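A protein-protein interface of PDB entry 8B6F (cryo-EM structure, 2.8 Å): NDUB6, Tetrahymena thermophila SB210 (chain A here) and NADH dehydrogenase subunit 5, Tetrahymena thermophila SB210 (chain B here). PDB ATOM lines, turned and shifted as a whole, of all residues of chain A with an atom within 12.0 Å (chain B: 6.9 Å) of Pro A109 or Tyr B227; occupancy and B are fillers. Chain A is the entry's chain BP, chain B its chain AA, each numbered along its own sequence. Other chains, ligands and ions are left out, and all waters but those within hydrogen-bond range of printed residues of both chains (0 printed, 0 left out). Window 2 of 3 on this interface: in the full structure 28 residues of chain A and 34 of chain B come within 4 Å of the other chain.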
ATOM      1  N   MET A 103      18.538  28.259  -5.090  1.00  0.00           N
ATOM      2  CA  MET A 103      18.044  26.888  -5.046  1.00  0.00           C
ATOM      3  C   MET A 103      16.862  26.670  -5.980  1.00  0.00           C
ATOM      4  O   MET A 103      16.578  25.523  -6.341  1.00  0.00           O
ATOM      5  CB  MET A 103      17.642  26.514  -3.619  1.00  0.00           C
ATOM      6  CG  MET A 103      18.809  26.226  -2.685  1.00  0.00           C
ATOM      7  SD  MET A 103      19.885  24.889  -3.233  1.00  0.00           S
ATOM      8  CE  MET A 103      21.245  25.811  -3.942  1.00  0.00           C
ATOM      9  N   SER A 105      16.784  27.402  -9.002  1.00  0.00           N
ATOM     10  CA  SER A 105      17.361  27.049 -10.293  1.00  0.00           C
ATOM     11  C   SER A 105      18.497  26.046 -10.129  1.00  0.00           C
ATOM     12  O   SER A 105      19.543  26.153 -10.770  1.00  0.00           O
ATOM     13  CB  SER A 105      17.842  28.297 -11.030  1.00  0.00           C
ATOM     14  OG  SER A 105      18.727  29.057 -10.229  1.00  0.00           O
ATOM     15  N   THR A 106      18.299  25.059  -9.262  1.00  0.00           N
ATOM     16  CA  THR A 106      19.262  23.991  -9.041  1.00  0.00           C
ATOM     17  C   THR A 106      18.754  22.711  -9.691  1.00  0.00           C
ATOM     18  O   THR A 106      17.546  22.454  -9.718  1.00  0.00           O
ATOM     19  CB  THR A 106      19.495  23.759  -7.545  1.00  0.00           C
ATOM     20  OG1 THR A 106      20.031  24.948  -6.953  1.00  0.00           O
ATOM     21  CG2 THR A 106      20.461  22.604  -7.309  1.00  0.00           C
ATOM     22  N   ALA A 107      19.679  21.915 -10.220  1.00  0.00           N
ATOM     23  CA  ALA A 107      19.360  20.655 -10.873  1.00  0.00           C
ATOM     24  C   ALA A 107      20.143  19.526 -10.220  1.00  0.00           C
ATOM     25  O   ALA A 107      21.323  19.684  -9.891  1.00  0.00           O
ATOM     26  CB  ALA A 107      19.678  20.711 -12.368  1.00  0.00           C
ATOM     27  N   LYS A 108      19.475  18.389 -10.026  1.00  0.00           N
ATOM     28  CA  LYS A 108      20.069  17.213  -9.418  1.00  0.00           C
ATOM     29  C   LYS A 108      19.644  15.990 -10.220  1.00  0.00           C
ATOM     30  O   LYS A 108      18.507  15.940 -10.710  1.00  0.00           O
ATOM     31  CB  LYS A 108      19.626  17.059  -7.955  1.00  0.00           C
ATOM     32  CG  LYS A 108      20.290  15.911  -7.212  1.00  0.00           C
ATOM     33  CD  LYS A 108      19.581  15.601  -5.904  1.00  0.00           C
ATOM     34  CE  LYS A 108      18.243  14.919  -6.148  1.00  0.00           C
ATOM     35  NZ  LYS A 108      17.642  14.399  -4.888  1.00  0.00           N
ATOM     36  N   PRO A 109      20.519  14.999 -10.378  1.00  0.00           N
ATOM     37  CA  PRO A 109      20.124  13.775 -11.078  1.00  0.00           C
ATOM     38  C   PRO A 109      19.200  12.932 -10.217  1.00  0.00           C
ATOM     39  O   PRO A 109      19.119  13.134  -8.998  1.00  0.00           O
ATOM     40  CB  PRO A 109      21.462  13.064 -11.328  1.00  0.00           C
ATOM     41  CG  PRO A 109      22.345  13.553 -10.252  1.00  0.00           C
ATOM     42  CD  PRO A 109      21.946  14.978 -10.011  1.00  0.00           C
ATOM     43  N   PRO A 110      18.483  11.980 -10.813  1.00  0.00           N
ATOM     44  CA  PRO A 110      17.587  11.130 -10.022  1.00  0.00           C
ATOM     45  C   PRO A 110      18.329  10.401  -8.910  1.00  0.00           C
ATOM     46  O   PRO A 110      19.557  10.291  -8.910  1.00  0.00           O
ATOM     47  CB  PRO A 110      17.025  10.145 -11.054  1.00  0.00           C
ATOM     48  CG  PRO A 110      17.164  10.838 -12.355  1.00  0.00           C
ATOM     49  CD  PRO A 110      18.404  11.672 -12.252  1.00  0.00           C
ATOM     50  N   ASN A 111      17.558   9.899  -7.950  1.00  0.00           N
ATOM     51  CA  ASN A 111      18.118   9.203  -6.799  1.00  0.00           C
ATOM     52  C   ASN A 111      18.461   7.764  -7.183  1.00  0.00           C
ATOM     53  O   ASN A 111      18.432   7.379  -8.354  1.00  0.00           O
ATOM     54  CB  ASN A 111      17.149   9.264  -5.621  1.00  0.00           C
ATOM     55  CG  ASN A 111      17.016  10.657  -5.046  1.00  0.00           C
ATOM     56  OD1 ASN A 111      17.952  11.451  -5.090  1.00  0.00           O
ATOM     57  ND2 ASN A 111      15.846  10.960  -4.496  1.00  0.00           N
ATOM     58  N   TYR A 112      18.799   6.950  -6.181  1.00  0.00           N
ATOM     59  CA  TYR A 112      19.246   5.587  -6.446  1.00  0.00           C
ATOM     60  C   TYR A 112      18.139   4.736  -7.059  1.00  0.00           C
ATOM     61  O   TYR A 112      18.389   3.975  -8.000  1.00  0.00           O
ATOM     62  CB  TYR A 112      19.750   4.950  -5.151  1.00  0.00           C
ATOM     63  CG  TYR A 112      20.058   3.479  -5.280  1.00  0.00           C
ATOM     64  CD1 TYR A 112      21.240   3.047  -5.861  1.00  0.00           C
ATOM     65  CD2 TYR A 112      19.166   2.524  -4.813  1.00  0.00           C
ATOM     66  CE1 TYR A 112      21.523   1.704  -5.979  1.00  0.00           C
ATOM     67  CE2 TYR A 112      19.440   1.178  -4.927  1.00  0.00           C
ATOM     68  CZ  TYR A 112      20.621   0.774  -5.509  1.00  0.00           C
ATOM     69  OH  TYR A 112      20.898  -0.565  -5.623  1.00  0.00           O
ATOM     70  N   GLY A 113      16.919   4.842  -6.544  1.00  0.00           N
ATOM     71  CA  GLY A 113      15.853   3.957  -6.972  1.00  0.00           C
ATOM     72  C   GLY A 113      14.937   4.538  -8.030  1.00  0.00           C
ATOM     73  O   GLY A 113      13.854   3.999  -8.272  1.00  0.00           O
ATOM     74  N   GLU A 114      15.356   5.621  -8.675  1.00  0.00           N
ATOM     75  CA  GLU A 114      14.512   6.357  -9.605  1.00  0.00           C
ATOM     76  C   GLU A 114      15.063   6.266 -11.021  1.00  0.00           C
ATOM     77  O   GLU A 114      16.278   6.326 -11.232  1.00  0.00           O
ATOM     78  CB  GLU A 114      14.402   7.826  -9.187  1.00  0.00           C
ATOM     79  CG  GLU A 114      13.849   8.024  -7.785  1.00  0.00           C
ATOM     80  CD  GLU A 114      13.913   9.467  -7.331  1.00  0.00           C
ATOM     81  OE1 GLU A 114      14.368  10.319  -8.121  1.00  0.00           O
ATOM     82  OE2 GLU A 114      13.512   9.749  -6.183  1.00  0.00           O
ATOM     83  N   TYR A 115      14.159   6.126 -11.986  1.00  0.00           N
ATOM     84  CA  TYR A 115      14.501   6.138 -13.400  1.00  0.00           C
ATOM     85  C   TYR A 115      13.633   7.166 -14.109  1.00  0.00           C
ATOM     86  O   TYR A 115      12.482   7.397 -13.728  1.00  0.00           O
ATOM     87  CB  TYR A 115      14.306   4.757 -14.046  1.00  0.00           C
ATOM     88  CG  TYR A 115      12.869   4.435 -14.388  1.00  0.00           C
ATOM     89  CD1 TYR A 115      12.007   3.910 -13.434  1.00  0.00           C
ATOM     90  CD2 TYR A 115      12.378   4.646 -15.669  1.00  0.00           C
ATOM     91  CE1 TYR A 115      10.695   3.612 -13.746  1.00  0.00           C
ATOM     92  CE2 TYR A 115      11.067   4.351 -15.990  1.00  0.00           C
ATOM     93  CZ  TYR A 115      10.232   3.835 -15.025  1.00  0.00           C
ATOM     94  OH  TYR A 115       8.928   3.540 -15.340  1.00  0.00           O
ATOM     95  N   VAL A 116      14.192   7.785 -15.142  1.00  0.00           N
ATOM     96  CA  VAL A 116      13.507   8.840 -15.879  1.00  0.00           C
ATOM     97  C   VAL A 116      12.691   8.200 -16.992  1.00  0.00           C
ATOM     98  O   VAL A 116      13.240   7.532 -17.873  1.00  0.00           O
ATOM     99  CB  VAL A 116      14.506   9.861 -16.445  1.00  0.00           C
ATOM    100  CG1 VAL A 116      13.791  10.910 -17.286  1.00  0.00           C
ATOM    101  CG2 VAL A 116      15.281  10.520 -15.318  1.00  0.00           C
ATOM    102  N   ASP A 117      11.384   8.402 -16.951  1.00  0.00           N
ATOM    103  CA  ASP A 117      10.508   7.883 -17.991  1.00  0.00           C
ATOM    104  C   ASP A 117      10.724   8.676 -19.274  1.00  0.00           C
ATOM    105  O   ASP A 117      10.565   9.903 -19.263  1.00  0.00           O
ATOM    106  CB  ASP A 117       9.055   7.972 -17.540  1.00  0.00           C
ATOM    107  CG  ASP A 117       8.090   7.446 -18.577  1.00  0.00           C
ATOM    108  OD1 ASP A 117       8.107   6.228 -18.846  1.00  0.00           O
ATOM    109  OD2 ASP A 117       7.309   8.249 -19.123  1.00  0.00           O
ATOM    110  N   VAL A 122       9.372  15.794 -18.122  1.00  0.00           N
ATOM    111  CA  VAL A 122      10.706  16.171 -17.665  1.00  0.00           C
ATOM    112  C   VAL A 122      11.779  15.627 -18.594  1.00  0.00           C
ATOM    113  O   VAL A 122      12.872  16.197 -18.692  1.00  0.00           O
ATOM    114  CB  VAL A 122      10.918  15.697 -16.219  1.00  0.00           C
ATOM    115  CG1 VAL A 122      12.328  16.014 -15.737  1.00  0.00           C
ATOM    116  CG2 VAL A 122       9.900  16.346 -15.331  1.00  0.00           C
ATOM    117  N   ALA A 123      11.499  14.525 -19.280  1.00  0.00           N
ATOM    118  CA  ALA A 123      12.486  13.955 -20.176  1.00  0.00           C
ATOM    119  C   ALA A 123      12.793  14.942 -21.301  1.00  0.00           C
ATOM    120  O   ALA A 123      11.915  15.693 -21.736  1.00  0.00           O
ATOM    121  CB  ALA A 123      11.982  12.637 -20.757  1.00  0.00           C
ATOM    122  N   PRO A 124      14.030  14.961 -21.793  1.00  0.00           N
ATOM    123  CA  PRO A 124      14.385  15.927 -22.839  1.00  0.00           C
ATOM    124  C   PRO A 124      13.538  15.736 -24.087  1.00  0.00           C
ATOM    125  O   PRO A 124      13.181  14.617 -24.457  1.00  0.00           O
ATOM    126  CB  PRO A 124      15.866  15.633 -23.107  1.00  0.00           C
ATOM    127  CG  PRO A 124      16.076  14.251 -22.623  1.00  0.00           C
ATOM    128  CD  PRO A 124      15.155  14.073 -21.461  1.00  0.00           C
ATOM    129  N   GLU B 169      18.676  16.991  -1.124  1.00  0.00           N
ATOM    130  CA  GLU B 169      17.943  17.618  -2.222  1.00  0.00           C
ATOM    131  C   GLU B 169      18.537  18.976  -2.599  1.00  0.00           C
ATOM    132  O   GLU B 169      18.666  19.284  -3.790  1.00  0.00           O
ATOM    133  CB  GLU B 169      16.467  17.748  -1.843  1.00  0.00           C
ATOM    134  CG  GLU B 169      15.607  18.483  -2.859  1.00  0.00           C
ATOM    135  CD  GLU B 169      15.400  17.711  -4.145  1.00  0.00           C
ATOM    136  OE1 GLU B 169      15.958  16.603  -4.274  1.00  0.00           O
ATOM    137  OE2 GLU B 169      14.673  18.216  -5.029  1.00  0.00           O
ATOM    138  N   LEU B 220      29.072  12.006  -0.394  1.00  0.00           N
ATOM    139  CA  LEU B 220      27.967  11.761  -1.316  1.00  0.00           C
ATOM    140  C   LEU B 220      28.404  11.908  -2.767  1.00  0.00           C
ATOM    141  O   LEU B 220      28.041  11.087  -3.617  1.00  0.00           O
ATOM    142  CB  LEU B 220      26.816  12.717  -1.010  1.00  0.00           C
ATOM    143  CG  LEU B 220      26.229  12.648   0.400  1.00  0.00           C
ATOM    144  CD1 LEU B 220      25.102  13.647   0.520  1.00  0.00           C
ATOM    145  CD2 LEU B 220      25.744  11.248   0.737  1.00  0.00           C
ATOM    146  N   ILE B 221      29.179  12.947  -3.076  1.00  0.00           N
ATOM    147  CA  ILE B 221      29.531  13.204  -4.467  1.00  0.00           C
ATOM    148  C   ILE B 221      30.470  12.126  -4.993  1.00  0.00           C
ATOM    149  O   ILE B 221      30.320  11.653  -6.125  1.00  0.00           O
ATOM    150  CB  ILE B 221      30.138  14.612  -4.608  1.00  0.00           C
ATOM    151  CG1 ILE B 221      29.123  15.673  -4.178  1.00  0.00           C
ATOM    152  CG2 ILE B 221      30.574  14.869  -6.044  1.00  0.00           C
ATOM    153  CD1 ILE B 221      29.727  17.033  -3.937  1.00  0.00           C
ATOM    154  N   GLU B 224      28.290   8.270  -3.809  1.00  0.00           N
ATOM    155  CA  GLU B 224      26.846   8.098  -3.918  1.00  0.00           C
ATOM    156  C   GLU B 224      26.270   8.622  -5.225  1.00  0.00           C
ATOM    157  O   GLU B 224      25.050   8.570  -5.408  1.00  0.00           O
ATOM    158  CB  GLU B 224      26.139   8.786  -2.745  1.00  0.00           C
ATOM    159  CG  GLU B 224      26.499   8.252  -1.378  1.00  0.00           C
ATOM    160  CD  GLU B 224      25.986   6.844  -1.170  1.00  0.00           C
ATOM    161  OE1 GLU B 224      25.231   6.355  -2.034  1.00  0.00           O
ATOM    162  OE2 GLU B 224      26.306   6.237  -0.133  1.00  0.00           O
ATOM    163  N   ASN B 225      27.105   9.133  -6.129  1.00  0.00           N
ATOM    164  CA  ASN B 225      26.654   9.617  -7.434  1.00  0.00           C
ATOM    165  C   ASN B 225      25.765  10.852  -7.297  1.00  0.00           C
ATOM    166  O   ASN B 225      24.778  11.004  -8.015  1.00  0.00           O
ATOM    167  CB  ASN B 225      25.928   8.521  -8.218  1.00  0.00           C
ATOM    168  CG  ASN B 225      26.819   7.335  -8.526  1.00  0.00           C
ATOM    169  OD1 ASN B 225      27.555   7.337  -9.510  1.00  0.00           O
ATOM    170  ND2 ASN B 225      26.751   6.311  -7.684  1.00  0.00           N
ATOM    171  N   TYR B 226      26.119  11.744  -6.377  1.00  0.00           N
ATOM    172  CA  TYR B 226      25.426  13.014  -6.201  1.00  0.00           C
ATOM    173  C   TYR B 226      26.235  14.126  -6.857  1.00  0.00           C
ATOM    174  O   TYR B 226      27.418  14.300  -6.549  1.00  0.00           O
ATOM    175  CB  TYR B 226      25.226  13.331  -4.718  1.00  0.00           C
ATOM    176  CG  TYR B 226      24.034  12.666  -4.073  1.00  0.00           C
ATOM    177  CD1 TYR B 226      22.798  13.295  -4.044  1.00  0.00           C
ATOM    178  CD2 TYR B 226      24.151  11.425  -3.465  1.00  0.00           C
ATOM    179  CE1 TYR B 226      21.707  12.699  -3.444  1.00  0.00           C
ATOM    180  CE2 TYR B 226      23.067  10.820  -2.860  1.00  0.00           C
ATOM    181  CZ  TYR B 226      21.848  11.462  -2.854  1.00  0.00           C
ATOM    182  OH  TYR B 226      20.765  10.867  -2.253  1.00  0.00           O
ATOM    183  N   TYR B 227      25.604  14.871  -7.758  1.00  0.00           N
ATOM    184  CA  TYR B 227      26.204  16.091  -8.271  1.00  0.00           C
ATOM    185  C   TYR B 227      25.095  17.096  -8.528  1.00  0.00           C
ATOM    186  O   TYR B 227      23.952  16.722  -8.801  1.00  0.00           O
ATOM    187  CB  TYR B 227      27.032  15.847  -9.540  1.00  0.00           C
ATOM    188  CG  TYR B 227      26.267  15.295 -10.717  1.00  0.00           C
ATOM    189  CD1 TYR B 227      25.583  16.137 -11.583  1.00  0.00           C
ATOM    190  CD2 TYR B 227      26.259  13.934 -10.981  1.00  0.00           C
ATOM    191  CE1 TYR B 227      24.894  15.636 -12.670  1.00  0.00           C
ATOM    192  CE2 TYR B 227      25.573  13.422 -12.064  1.00  0.00           C
ATOM    193  CZ  TYR B 227      24.893  14.277 -12.905  1.00  0.00           C
ATOM    194  OH  TYR B 227      24.210  13.768 -13.984  1.00  0.00           O
ATOM    195  N   TYR B 228      25.440  18.374  -8.429  1.00  0.00           N
ATOM    196  CA  TYR B 228      24.473  19.453  -8.518  1.00  0.00           C
ATOM    197  C   TYR B 228      24.884  20.433  -9.606  1.00  0.00           C
ATOM    198  O   TYR B 228      26.072  20.635  -9.868  1.00  0.00           O
ATOM    199  CB  TYR B 228      24.344  20.195  -7.184  1.00  0.00           C
ATOM    200  CG  TYR B 228      24.099  19.285  -6.006  1.00  0.00           C
ATOM    201  CD1 TYR B 228      22.814  18.883  -5.670  1.00  0.00           C
ATOM    202  CD2 TYR B 228      25.152  18.833  -5.227  1.00  0.00           C
ATOM    203  CE1 TYR B 228      22.588  18.053  -4.594  1.00  0.00           C
ATOM    204  CE2 TYR B 228      24.937  18.003  -4.148  1.00  0.00           C
ATOM    205  CZ  TYR B 228      23.651  17.617  -3.837  1.00  0.00           C
ATOM    206  OH  TYR B 228      23.431  16.789  -2.763  1.00  0.00           O
ATOM    207  N   TYR B 229      23.883  21.044 -10.235  1.00  0.00           N
ATOM    208  CA  TYR B 229      24.088  22.110 -11.209  1.00  0.00           C
ATOM    209  C   TYR B 229      23.261  23.303 -10.743  1.00  0.00           C
ATOM    210  O   TYR B 229      22.034  23.305 -10.875  1.00  0.00           O
ATOM    211  CB  TYR B 229      23.692  21.669 -12.612  1.00  0.00           C
ATOM    212  CG  TYR B 229      23.778  22.773 -13.636  1.00  0.00           C
ATOM    213  CD1 TYR B 229      25.000  23.174 -14.154  1.00  0.00           C
ATOM    214  CD2 TYR B 229      22.633  23.416 -14.085  1.00  0.00           C
ATOM    215  CE1 TYR B 229      25.080  24.183 -15.089  1.00  0.00           C
ATOM    216  CE2 TYR B 229      22.701  24.426 -15.019  1.00  0.00           C
ATOM    217  CZ  TYR B 229      23.927  24.805 -15.518  1.00  0.00           C
ATOM    218  OH  TYR B 229      24.001  25.812 -16.450  1.00  0.00           O
ATOM    219  N   LEU B 249      28.908  23.884 -11.252  1.00  0.00           N
ATOM    220  CA  LEU B 249      28.755  22.442 -11.427  1.00  0.00           C
ATOM    221  C   LEU B 249      29.548  21.747 -10.326  1.00  0.00           C
ATOM    222  O   LEU B 249      30.779  21.689 -10.380  1.00  0.00           O
ATOM    223  CB  LEU B 249      29.231  22.012 -12.811  1.00  0.00           C
ATOM    224  CG  LEU B 249      29.278  20.510 -13.087  1.00  0.00           C
ATOM    225  CD1 LEU B 249      27.887  19.900 -13.043  1.00  0.00           C
ATOM    226  CD2 LEU B 249      29.943  20.259 -14.423  1.00  0.00           C
ATOM    227  N   ILE B 250      28.843  21.226  -9.329  1.00  0.00           N
ATOM    228  CA  ILE B 250      29.462  20.476  -8.240  1.00  0.00           C
ATOM    229  C   ILE B 250      29.331  19.005  -8.622  1.00  0.00           C
ATOM    230  O   ILE B 250      28.369  18.326  -8.264  1.00  0.00           O
ATOM    231  CB  ILE B 250      28.817  20.788  -6.892  1.00  0.00           C
ATOM    232  CG1 ILE B 250      28.790  22.303  -6.664  1.00  0.00           C
ATOM    233  CG2 ILE B 250      29.580  20.086  -5.780  1.00  0.00           C
ATOM    234  CD1 ILE B 250      28.115  22.728  -5.375  1.00  0.00           C
ATOM    235  N   ASP B 251      30.322  18.511  -9.353  1.00  0.00           N
ATOM    236  CA  ASP B 251      30.401  17.130  -9.801  1.00  0.00           C
ATOM    237  C   ASP B 251      31.580  16.454  -9.108  1.00  0.00           C
ATOM    238  O   ASP B 251      32.231  17.036  -8.237  1.00  0.00           O
ATOM    239  CB  ASP B 251      30.534  17.079 -11.325  1.00  0.00           C
ATOM    240  CG  ASP B 251      30.131  15.739 -11.906  1.00  0.00           C
ATOM    241  OD1 ASP B 251      30.226  14.725 -11.185  1.00  0.00           O
ATOM    242  OD2 ASP B 251      29.719  15.697 -13.085  1.00  0.00           O
ATOM    243  N   LEU B 252      31.852  15.204  -9.489  1.00  0.00           N
ATOM    244  CA  LEU B 252      33.027  14.528  -8.950  1.00  0.00           C
ATOM    245  C   LEU B 252      34.304  15.241  -9.373  1.00  0.00           C
ATOM    246  O   LEU B 252      35.224  15.413  -8.567  1.00  0.00           O
ATOM    247  CB  LEU B 252      33.055  13.065  -9.392  1.00  0.00           C
ATOM    248  CG  LEU B 252      34.270  12.259  -8.917  1.00  0.00           C
ATOM    249  CD1 LEU B 252      33.894  10.812  -8.694  1.00  0.00           C
ATOM    250  CD2 LEU B 252      35.434  12.335  -9.896  1.00  0.00           C
ATOM    251  N   LEU B 367      28.569  20.766 -19.838  1.00  0.00           N
ATOM    252  CA  LEU B 367      27.967  19.463 -20.104  1.00  0.00           C
ATOM    253  C   LEU B 367      27.537  19.342 -21.556  1.00  0.00           C
ATOM    254  O   LEU B 367      27.752  18.305 -22.192  1.00  0.00           O
ATOM    255  CB  LEU B 367      26.775  19.229 -19.179  1.00  0.00           C
ATOM    256  CG  LEU B 367      27.100  18.655 -17.800  1.00  0.00           C
ATOM    257  CD1 LEU B 367      28.036  19.564 -17.042  1.00  0.00           C
ATOM    258  CD2 LEU B 367      25.827  18.424 -17.010  1.00  0.00           C
ATOM    259  N   ASP B 676      30.327   8.043 -11.203  1.00  0.00           N
ATOM    260  CA  ASP B 676      30.513   8.086 -12.644  1.00  0.00           C
ATOM    261  C   ASP B 676      31.414   9.250 -13.036  1.00  0.00           C
ATOM    262  O   ASP B 676      31.278  10.363 -12.525  1.00  0.00           O
ATOM    263  CB  ASP B 676      29.154   8.218 -13.330  1.00  0.00           C
ATOM    264  CG  ASP B 676      29.237   8.063 -14.830  1.00  0.00           C
ATOM    265  OD1 ASP B 676      30.318   7.707 -15.342  1.00  0.00           O
ATOM    266  OD2 ASP B 676      28.212   8.312 -15.498  1.00  0.00           O
ATOM    267  N   LYS B 678      31.645  10.163 -16.314  1.00  0.00           N
ATOM    268  CA  LYS B 678      31.051  10.741 -17.516  1.00  0.00           C
ATOM    269  C   LYS B 678      31.990  10.651 -18.716  1.00  0.00           C
ATOM    270  O   LYS B 678      32.003  11.537 -19.573  1.00  0.00           O
ATOM    271  CB  LYS B 678      30.634  12.194 -17.276  1.00  0.00           C
ATOM    272  CG  LYS B 678      29.816  12.405 -16.007  1.00  0.00           C
ATOM    273  CD  LYS B 678      28.541  11.572 -16.012  1.00  0.00           C
ATOM    274  CE  LYS B 678      27.734  11.791 -14.743  1.00  0.00           C
ATOM    275  NZ  LYS B 678      26.476  10.993 -14.735  1.00  0.00           N
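The side-chain carboxylate (OE1) of Glu B169 is in salt-bridge range of the side-chain amino group (NZ) of Lys A108, at 2.8 Å.
N of Ala A107 lies within hydrogen-bond range of O of Tyr B229, at 2.8 Å.
The side-chain amide oxygen (OD1) of Asn A111 lies within hydrogen-bond range of the side-chain amino group (NZ) of Lys A108 (3.0 Å).
The backbone NH of Ile B250 sits at hydrogen-bond distance from the backbone carbonyl oxygen of Tyr B228, 2.9 Å away.
The side-chain sulfur of Met A103 lies close to the side-chain hydroxyl of Thr A106 (3.7 Å).
Tyr B229 touches Ser A105.
Thr A106 touches Tyr B229.
Tyr B228 touches Ala A107 (CA to O, 3.4 Å).
Lys A108 touches Tyr B227 (CA to O, 3.96 Å).
Pro A109 touches Tyr B227.
Pro A109 touches just one residue of chain B: Tyr B227 (2.9 Å).
No residue of chain A comes within 4 Å of Ile B221.
Tyr B226 touches none of the printed residues of chain A.
Of chain A, only Ala A107 comes within 4 Å of Tyr B228.
No residue of chain A comes within 4 Å of Ile B250.
No residue of chain A comes within 4 Å of Asp B251.
Of the printed residues of chain A, Tyr B229 touches Ser A105, Thr A106 and Ala A107.
Of the printed residues of chain B, Lys A108 touches Glu B169 and Tyr B227.
Of the printed residues of chain A, Glu B169 touches Lys A108.
Of the printed residues of chain B, Ser A105 touches Tyr B229.
Of the printed residues of chain B, Thr A106 touches Tyr B229 (3.4 Å).
Ala A123 touches none of the printed residues of chain B.
Pro A124 touches none of the printed residues of chain B.
The nearest residue of chain B that does not touch Pro A109 is Asn B225 (4.2 Å).
The nearest residue of chain A that does not touch Tyr B227 is Ala A107 (4.1 Å).
Of the 16 printed residues of chain B, 4 touch a printed residue of chain A.
Hydrophobic or aromatic side chains of chain B within 4 Å of the printed part of chain A: Tyr B227.
Of the 17 printed residues of chain A, 5 touch a printed residue of chain B.
Among the printed residues, Asp or Glu carboxylates within 4 Å of a Lys or Arg side-chain nitrogen of the other chain: Lys A108 with Glu B169 (2.8 Å).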
